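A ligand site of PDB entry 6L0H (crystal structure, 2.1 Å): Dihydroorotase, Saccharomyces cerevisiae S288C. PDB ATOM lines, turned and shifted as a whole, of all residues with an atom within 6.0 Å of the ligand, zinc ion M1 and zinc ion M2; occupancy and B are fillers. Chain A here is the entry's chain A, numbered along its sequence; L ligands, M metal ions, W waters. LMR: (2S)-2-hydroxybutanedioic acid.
OG1 of Thr 106 is in hydrogen-bond range of O1A of the ligand (2.6 Å).
O4A of the ligand lies within hydrogen-bond range of OG1 of Thr 105 (2.7 Å).
O1B of the ligand lies within salt-bridge range of NH1 of Arg 18.
The backbone carbonyl oxygen of Ala 275 is in hydrogen-bond range of an oxygen (O2) of the ligand.
The side-chain amide nitrogen (ND2) of Asn 43 sits at hydrogen-bond distance from an oxygen (O1B) of the ligand (2.9 Å).
A ring nitrogen (NE2) of His 262 is in hydrogen-bond range of an oxygen (O1A) of the ligand, 3.2 Å away.
OE1 of Glu 179 lies within hydrogen-bond range of ND1 of His 14, 2.9 Å away.
NZ of KCX 98 sits at hydrogen-bond distance from the side-chain sulfur (SD) of Met 41, at 3.5 Å.
NZ of KCX 98 is in hydrogen-bond range of the side-chain hydroxyl (OH) of Tyr 100, at 3.0 Å.
A ring nitrogen (ND1) of His 16 sits at hydrogen-bond distance from the side-chain amide oxygen (OD1) of Asn 43 (3.0 Å).
O of Thr 106 sits at hydrogen-bond distance from ND2 of Asn 43 (3.1 Å).
The guanidinium group (NH2) of Arg 18 lies close to a ring nitrogen (NE2) of His 262 (3.4 Å).
The guanidinium group of Arg 18 is in hydrogen-bond range of the backbone carbonyl oxygen of Pro 261, 2.9 Å away.
O of Ala 275 is in hydrogen-bond range of NE2 of His 262.
O of Lys 230 lies close to O4A of the ligand (3.5 Å).
Ala 260 touches the ligand.
Hydrophobic or aromatic side chains within 4 Å of the ligand: His 16, His 137, His 180, Ala 260 and His 262.
Within 4 Å of the ligand: His 14, His 16, Arg 18, Asn 43, KCX 98, Thr 105, Thr 106, His 137, His 180, Lys 230, Asp 258, Ala 260, His 262 and Ala 275.
The nearest printed residue that does not touch the ligand is Gly 276 (4.1 Å).
Four residues have an atom within 4 Å of zinc ion M1: His 14, His 16, KCX 98 and Asp 258.
The nearest printed residue that does not touch zinc ion M1 is His 180 (4.3 Å).
Three residues have an atom within 4 Å of zinc ion M2: KCX 98, His 137 and His 180.
Along chain A the residues within 4 Å of zinc ion M2 span positions 98 to 180.
Zinc ion M1 is bound by O4B of the ligand (1.9 Å), OD1 of Asp 258 (2.0 Å), NE2 of His 14 (2.0 Å), NE2 of His 16 (2.0 Å) and OQ1 of KCX 98 (2.2 Å).
Zinc ion M2 is bound by OQ2 of KCX 98, ND1 of His 137, NE2 of His 180 and O4B of the ligand.
Zinc ion M2 has four donor atoms within binding distance.
Slightly farther from zinc ion M2 lies O4A of the ligand (2.8 Å).
Water W1 lies within hydrogen-bond range of an oxygen (O2) of the ligand (2.8 Å), the backbone NH (N) of Lys 230 (3.0 Å) and the side-chain carboxylate (OD2) of Asp 258 (3.3 Å).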
ATOM      1  N   HIS A  14     -25.925 -28.546   4.838  1.00  0.00           N
ATOM      2  CA  HIS A  14     -24.496 -28.555   4.469  1.00  0.00           C
ATOM      3  C   HIS A  14     -24.284 -27.493   3.380  1.00  0.00           C
ATOM      4  O   HIS A  14     -24.446 -27.784   2.199  1.00  0.00           O
ATOM      5  CB  HIS A  14     -24.069 -29.937   4.033  1.00  0.00           C
ATOM      6  CG  HIS A  14     -22.593 -30.100   3.895  1.00  0.00           C
ATOM      7  ND1 HIS A  14     -21.922 -31.232   4.323  1.00  0.00           N
ATOM      8  CD2 HIS A  14     -21.650 -29.295   3.350  1.00  0.00           C
ATOM      9  CE1 HIS A  14     -20.635 -31.098   4.049  1.00  0.00           C
ATOM     10  NE2 HIS A  14     -20.450 -29.929   3.458  1.00  0.00           N
ATOM     11  N   HIS A  16     -21.895 -24.130   1.876  1.00  0.00           N
ATOM     12  CA  HIS A  16     -20.722 -23.260   1.785  1.00  0.00           C
ATOM     13  C   HIS A  16     -21.140 -21.948   1.144  1.00  0.00           C
ATOM     14  O   HIS A  16     -21.725 -21.941   0.060  1.00  0.00           O
ATOM     15  CB  HIS A  16     -19.596 -23.902   0.975  1.00  0.00           C
ATOM     16  CG  HIS A  16     -19.094 -25.163   1.593  1.00  0.00           C
ATOM     17  ND1 HIS A  16     -18.123 -25.169   2.560  1.00  0.00           N
ATOM     18  CD2 HIS A  16     -19.454 -26.451   1.407  1.00  0.00           C
ATOM     19  CE1 HIS A  16     -17.890 -26.416   2.942  1.00  0.00           C
ATOM     20  NE2 HIS A  16     -18.699 -27.216   2.261  1.00  0.00           N
ATOM     21  N   ARG A  18     -18.774 -19.009   1.530  1.00  0.00           N
ATOM     22  CA  ARG A  18     -17.528 -18.251   1.322  1.00  0.00           C
ATOM     23  C   ARG A  18     -17.599 -16.890   2.030  1.00  0.00           C
ATOM     24  O   ARG A  18     -18.300 -16.728   3.036  1.00  0.00           O
ATOM     25  CB  ARG A  18     -17.213 -18.140  -0.172  1.00  0.00           C
ATOM     26  CG  ARG A  18     -17.365 -19.415  -0.987  1.00  0.00           C
ATOM     27  CD  ARG A  18     -16.533 -20.573  -0.467  1.00  0.00           C
ATOM     28  NE  ARG A  18     -16.604 -21.666  -1.436  1.00  0.00           N
ATOM     29  CZ  ARG A  18     -16.304 -22.936  -1.184  1.00  0.00           C
ATOM     30  NH1 ARG A  18     -15.893 -23.323   0.042  1.00  0.00           N
ATOM     31  NH2 ARG A  18     -16.398 -23.821  -2.166  1.00  0.00           N
ATOM     32  N   MET A  41     -21.087 -24.180   6.829  1.00  0.00           N
ATOM     33  CA  MET A  41     -19.807 -24.834   7.069  1.00  0.00           C
ATOM     34  C   MET A  41     -18.701 -23.810   7.294  1.00  0.00           C
ATOM     35  O   MET A  41     -18.784 -22.668   6.828  1.00  0.00           O
ATOM     36  CB  MET A  41     -19.466 -25.767   5.916  1.00  0.00           C
ATOM     37  CG  MET A  41     -20.282 -27.044   5.941  1.00  0.00           C
ATOM     38  SD  MET A  41     -20.257 -27.924   7.552  1.00  0.00           S
ATOM     39  CE  MET A  41     -21.450 -29.241   7.270  1.00  0.00           C
ATOM     40  N   ASN A  43     -15.132 -23.793   6.728  1.00  0.00           N
ATOM     41  CA  ASN A  43     -13.795 -23.838   6.123  1.00  0.00           C
ATOM     42  C   ASN A  43     -13.494 -22.563   5.319  1.00  0.00           C
ATOM     43  O   ASN A  43     -13.251 -22.596   4.110  1.00  0.00           O
ATOM     44  CB  ASN A  43     -13.648 -25.080   5.264  1.00  0.00           C
ATOM     45  CG  ASN A  43     -14.609 -25.088   4.100  1.00  0.00           C
ATOM     46  OD1 ASN A  43     -15.677 -24.472   4.153  1.00  0.00           O
ATOM     47  ND2 ASN A  43     -14.234 -25.795   3.022  1.00  0.00           N
ATOM     48  N   KCX A  98     -17.277 -28.896  12.801  1.00  0.00           N
ATOM     49  CA  KCX A  98     -17.071 -29.667  11.580  1.00  0.00           C
ATOM     50  CB  KCX A  98     -17.430 -28.815  10.347  1.00  0.00           C
ATOM     51  CG  KCX A  98     -17.010 -29.434   9.018  1.00  0.00           C
ATOM     52  CD  KCX A  98     -17.837 -30.689   8.722  1.00  0.00           C
ATOM     53  CE  KCX A  98     -17.619 -31.188   7.301  1.00  0.00           C
ATOM     54  NZ  KCX A  98     -17.761 -30.059   6.364  1.00  0.00           N
ATOM     55  C   KCX A  98     -15.639 -30.149  11.484  1.00  0.00           C
ATOM     56  O   KCX A  98     -14.698 -29.365  11.629  1.00  0.00           O
ATOM     57  CX  KCX A  98     -17.651 -30.234   5.042  1.00  0.00           C
ATOM     58  OQ1 KCX A  98     -17.754 -29.255   4.286  1.00  0.00           O
ATOM     59  OQ2 KCX A  98     -17.447 -31.375   4.595  1.00  0.00           O
ATOM     60  N   TYR A 100     -12.599 -31.613   9.298  1.00  0.00           N
ATOM     61  CA  TYR A 100     -11.976 -31.859   7.991  1.00  0.00           C
ATOM     62  C   TYR A 100     -10.685 -32.626   8.212  1.00  0.00           C
ATOM     63  O   TYR A 100      -9.786 -32.094   8.874  1.00  0.00           O
ATOM     64  CB  TYR A 100     -11.684 -30.555   7.244  1.00  0.00           C
ATOM     65  CG  TYR A 100     -12.902 -29.755   6.833  1.00  0.00           C
ATOM     66  CD1 TYR A 100     -13.533 -29.989   5.617  1.00  0.00           C
ATOM     67  CD2 TYR A 100     -13.416 -28.771   7.652  1.00  0.00           C
ATOM     68  CE1 TYR A 100     -14.632 -29.274   5.238  1.00  0.00           C
ATOM     69  CE2 TYR A 100     -14.521 -28.024   7.274  1.00  0.00           C
ATOM     70  CZ  TYR A 100     -15.126 -28.305   6.056  1.00  0.00           C
ATOM     71  OH  TYR A 100     -16.233 -27.595   5.656  1.00  0.00           O
ATOM     72  N   VAL A 104      -7.731 -33.414   2.411  1.00  0.00           N
ATOM     73  CA  VAL A 104      -8.674 -34.149   1.553  1.00  0.00           C
ATOM     74  C   VAL A 104      -9.641 -33.255   0.780  1.00  0.00           C
ATOM     75  O   VAL A 104     -10.318 -33.770  -0.127  1.00  0.00           O
ATOM     76  CB  VAL A 104      -9.493 -35.216   2.312  1.00  0.00           C
ATOM     77  CG1 VAL A 104      -8.564 -36.200   3.012  1.00  0.00           C
ATOM     78  CG2 VAL A 104     -10.484 -34.568   3.311  1.00  0.00           C
ATOM     79  N   THR A 105      -9.754 -31.954   1.106  1.00  0.00           N
ATOM     80  CA  THR A 105     -10.685 -31.094   0.354  1.00  0.00           C
ATOM     81  C   THR A 105     -10.338 -29.619   0.562  1.00  0.00           C
ATOM     82  O   THR A 105      -9.326 -29.269   1.181  1.00  0.00           O
ATOM     83  CB  THR A 105     -12.147 -31.362   0.720  1.00  0.00           C
ATOM     84  OG1 THR A 105     -12.989 -30.705  -0.218  1.00  0.00           O
ATOM     85  CG2 THR A 105     -12.475 -30.881   2.138  1.00  0.00           C
ATOM     86  N   THR A 106     -11.212 -28.737   0.042  1.00  0.00           N
ATOM     87  CA  THR A 106     -10.997 -27.291   0.108  1.00  0.00           C
ATOM     88  C   THR A 106     -10.719 -26.804   1.536  1.00  0.00           C
ATOM     89  O   THR A 106     -11.489 -27.060   2.460  1.00  0.00           O
ATOM     90  CB  THR A 106     -12.224 -26.545  -0.451  1.00  0.00           C
ATOM     91  OG1 THR A 106     -12.456 -26.930  -1.817  1.00  0.00           O
ATOM     92  CG2 THR A 106     -12.027 -25.028  -0.400  1.00  0.00           C
ATOM     93  N   HIS A 137     -16.434 -34.788   7.666  1.00  0.00           N
ATOM     94  CA  HIS A 137     -16.061 -35.087   6.282  1.00  0.00           C
ATOM     95  C   HIS A 137     -15.298 -36.394   6.378  1.00  0.00           C
ATOM     96  O   HIS A 137     -14.084 -36.425   6.592  1.00  0.00           O
ATOM     97  CB  HIS A 137     -15.231 -33.987   5.630  1.00  0.00           C
ATOM     98  CG  HIS A 137     -14.894 -34.244   4.194  1.00  0.00           C
ATOM     99  ND1 HIS A 137     -15.266 -33.399   3.162  1.00  0.00           N
ATOM    100  CD2 HIS A 137     -14.220 -35.272   3.616  1.00  0.00           C
ATOM    101  CE1 HIS A 137     -14.849 -33.897   2.017  1.00  0.00           C
ATOM    102  NE2 HIS A 137     -14.207 -35.036   2.253  1.00  0.00           N
ATOM    103  N   GLU A 179     -21.205 -36.555   6.825  1.00  0.00           N
ATOM    104  CA  GLU A 179     -21.665 -35.638   5.791  1.00  0.00           C
ATOM    105  C   GLU A 179     -21.504 -36.260   4.403  1.00  0.00           C
ATOM    106  O   GLU A 179     -20.688 -37.162   4.196  1.00  0.00           O
ATOM    107  CB  GLU A 179     -20.885 -34.309   5.884  1.00  0.00           C
ATOM    108  CG  GLU A 179     -21.122 -33.500   7.183  1.00  0.00           C
ATOM    109  CD  GLU A 179     -22.557 -32.974   7.316  1.00  0.00           C
ATOM    110  OE1 GLU A 179     -23.245 -32.833   6.289  1.00  0.00           O
ATOM    111  OE2 GLU A 179     -23.011 -32.654   8.447  1.00  0.00           O
ATOM    112  N   HIS A 180     -22.327 -35.796   3.461  1.00  0.00           N
ATOM    113  CA  HIS A 180     -22.329 -36.153   2.040  1.00  0.00           C
ATOM    114  C   HIS A 180     -21.807 -37.562   1.751  1.00  0.00           C
ATOM    115  O   HIS A 180     -20.714 -37.736   1.196  1.00  0.00           O
ATOM    116  CB  HIS A 180     -21.551 -35.111   1.208  1.00  0.00           C
ATOM    117  CG  HIS A 180     -20.227 -34.711   1.784  1.00  0.00           C
ATOM    118  ND1 HIS A 180     -19.319 -35.617   2.285  1.00  0.00           N
ATOM    119  CD2 HIS A 180     -19.644 -33.491   1.928  1.00  0.00           C
ATOM    120  CE1 HIS A 180     -18.235 -34.981   2.720  1.00  0.00           C
ATOM    121  NE2 HIS A 180     -18.410 -33.696   2.509  1.00  0.00           N
ATOM    122  N   CYS A 229     -15.829 -33.050  -7.190  1.00  0.00           N
ATOM    123  CA  CYS A 229     -16.050 -32.644  -5.809  1.00  0.00           C
ATOM    124  C   CYS A 229     -15.457 -33.708  -4.891  1.00  0.00           C
ATOM    125  O   CYS A 229     -14.998 -34.753  -5.347  1.00  0.00           O
ATOM    126  CB  CYS A 229     -17.554 -32.460  -5.523  1.00  0.00           C
ATOM    127  SG  CYS A 229     -18.474 -34.023  -5.657  1.00  0.00           S
ATOM    128  N   LYS A 230     -15.410 -33.390  -3.596  1.00  0.00           N
ATOM    129  CA  LYS A 230     -15.062 -34.343  -2.536  1.00  0.00           C
ATOM    130  C   LYS A 230     -16.265 -34.598  -1.623  1.00  0.00           C
ATOM    131  O   LYS A 230     -16.981 -33.648  -1.278  1.00  0.00           O
ATOM    132  CB  LYS A 230     -13.901 -33.820  -1.689  1.00  0.00           C
ATOM    133  CG  LYS A 230     -12.621 -33.629  -2.462  1.00  0.00           C
ATOM    134  CD  LYS A 230     -12.297 -34.888  -3.242  1.00  0.00           C
ATOM    135  CE  LYS A 230     -10.890 -35.310  -3.023  1.00  0.00           C
ATOM    136  NZ  LYS A 230     -10.693 -36.214  -1.863  1.00  0.00           N
ATOM    137  N   PRO A 231     -16.533 -35.854  -1.199  1.00  0.00           N
ATOM    138  CA  PRO A 231     -15.933 -37.076  -1.739  1.00  0.00           C
ATOM    139  C   PRO A 231     -16.333 -37.200  -3.205  1.00  0.00           C
ATOM    140  O   PRO A 231     -17.374 -36.687  -3.627  1.00  0.00           O
ATOM    141  CB  PRO A 231     -16.533 -38.214  -0.889  1.00  0.00           C
ATOM    142  CG  PRO A 231     -17.250 -37.537   0.260  1.00  0.00           C
ATOM    143  CD  PRO A 231     -17.614 -36.164  -0.256  1.00  0.00           C
ATOM    144  N   ASP A 258     -24.005 -29.707   0.186  1.00  0.00           N
ATOM    145  CA  ASP A 258     -22.585 -29.372   0.001  1.00  0.00           C
ATOM    146  C   ASP A 258     -22.393 -28.517  -1.250  1.00  0.00           C
ATOM    147  O   ASP A 258     -21.402 -28.660  -2.004  1.00  0.00           O
ATOM    148  CB  ASP A 258     -21.694 -30.607  -0.044  1.00  0.00           C
ATOM    149  CG  ASP A 258     -20.199 -30.245   0.053  1.00  0.00           C
ATOM    150  OD1 ASP A 258     -19.882 -29.237   0.702  1.00  0.00           O
ATOM    151  OD2 ASP A 258     -19.352 -30.959  -0.534  1.00  0.00           O
ATOM    152  N   ALA A 260     -20.891 -25.849  -3.042  1.00  0.00           N
ATOM    153  CA  ALA A 260     -19.547 -25.359  -2.786  1.00  0.00           C
ATOM    154  C   ALA A 260     -19.158 -24.462  -3.956  1.00  0.00           C
ATOM    155  O   ALA A 260     -18.611 -24.940  -4.960  1.00  0.00           O
ATOM    156  CB  ALA A 260     -18.578 -26.530  -2.614  1.00  0.00           C
ATOM    157  N   PRO A 261     -19.463 -23.160  -3.885  1.00  0.00           N
ATOM    158  CA  PRO A 261     -19.211 -22.290  -5.040  1.00  0.00           C
ATOM    159  C   PRO A 261     -17.739 -21.966  -5.225  1.00  0.00           C
ATOM    160  O   PRO A 261     -17.003 -21.762  -4.264  1.00  0.00           O
ATOM    161  CB  PRO A 261     -20.042 -21.036  -4.755  1.00  0.00           C
ATOM    162  CG  PRO A 261     -20.493 -21.136  -3.311  1.00  0.00           C
ATOM    163  CD  PRO A 261     -20.098 -22.463  -2.757  1.00  0.00           C
ATOM    164  N   HIS A 262     -17.291 -21.996  -6.490  1.00  0.00           N
ATOM    165  CA  HIS A 262     -15.966 -21.563  -6.931  1.00  0.00           C
ATOM    166  C   HIS A 262     -16.145 -20.720  -8.195  1.00  0.00           C
ATOM    167  O   HIS A 262     -16.930 -21.101  -9.087  1.00  0.00           O
ATOM    168  CB  HIS A 262     -15.035 -22.731  -7.265  1.00  0.00           C
ATOM    169  CG  HIS A 262     -14.757 -23.649  -6.116  1.00  0.00           C
ATOM    170  ND1 HIS A 262     -13.911 -23.299  -5.077  1.00  0.00           N
ATOM    171  CD2 HIS A 262     -15.200 -24.903  -5.843  1.00  0.00           C
ATOM    172  CE1 HIS A 262     -13.848 -24.307  -4.217  1.00  0.00           C
ATOM    173  NE2 HIS A 262     -14.621 -25.282  -4.659  1.00  0.00           N
ATOM    174  N   ALA A 275     -12.162 -28.492  -5.783  1.00  0.00           N
ATOM    175  CA  ALA A 275     -13.260 -29.446  -5.634  1.00  0.00           C
ATOM    176  C   ALA A 275     -14.524 -28.729  -5.162  1.00  0.00           C
ATOM    177  O   ALA A 275     -14.487 -27.939  -4.215  1.00  0.00           O
ATOM    178  CB  ALA A 275     -12.882 -30.555  -4.647  1.00  0.00           C
ATOM    179  N   GLY A 276     -15.653 -29.030  -5.791  1.00  0.00           N
ATOM    180  CA  GLY A 276     -16.927 -28.474  -5.380  1.00  0.00           C
ATOM    181  C   GLY A 276     -17.889 -28.252  -6.533  1.00  0.00           C
ATOM    182  O   GLY A 276     -17.491 -27.849  -7.637  1.00  0.00           O
HETATM  183  C1  LMR L   1     -15.515 -26.750  -0.604  1.00  0.00           C
HETATM  184  O1A LMR L   1     -15.015 -26.287  -1.656  1.00  0.00           O
HETATM  185  O1B LMR L   1     -15.598 -26.069   0.457  1.00  0.00           O
HETATM  186  C2  LMR L   1     -16.017 -28.193  -0.606  1.00  0.00           C
HETATM  187  O2  LMR L   1     -15.320 -28.886  -1.599  1.00  0.00           O
HETATM  188  C3  LMR L   1     -15.696 -28.699   0.788  1.00  0.00           C
HETATM  189  C4  LMR L   1     -16.268 -30.096   0.990  1.00  0.00           C
HETATM  190  O4A LMR L   1     -15.569 -31.083   0.639  1.00  0.00           O
HETATM  191  O4B LMR L   1     -17.403 -30.237   1.532  1.00  0.00           O
HETATM  192 ZN    ZN M   1     -18.845 -29.256   2.394  1.00  0.00          ZN
HETATM  193 ZN    ZN M   2     -16.935 -32.186   2.795  1.00  0.00          ZN
HETATM  194  O   HOH W   1     -16.833 -30.954  -2.621  1.00  0.00           O
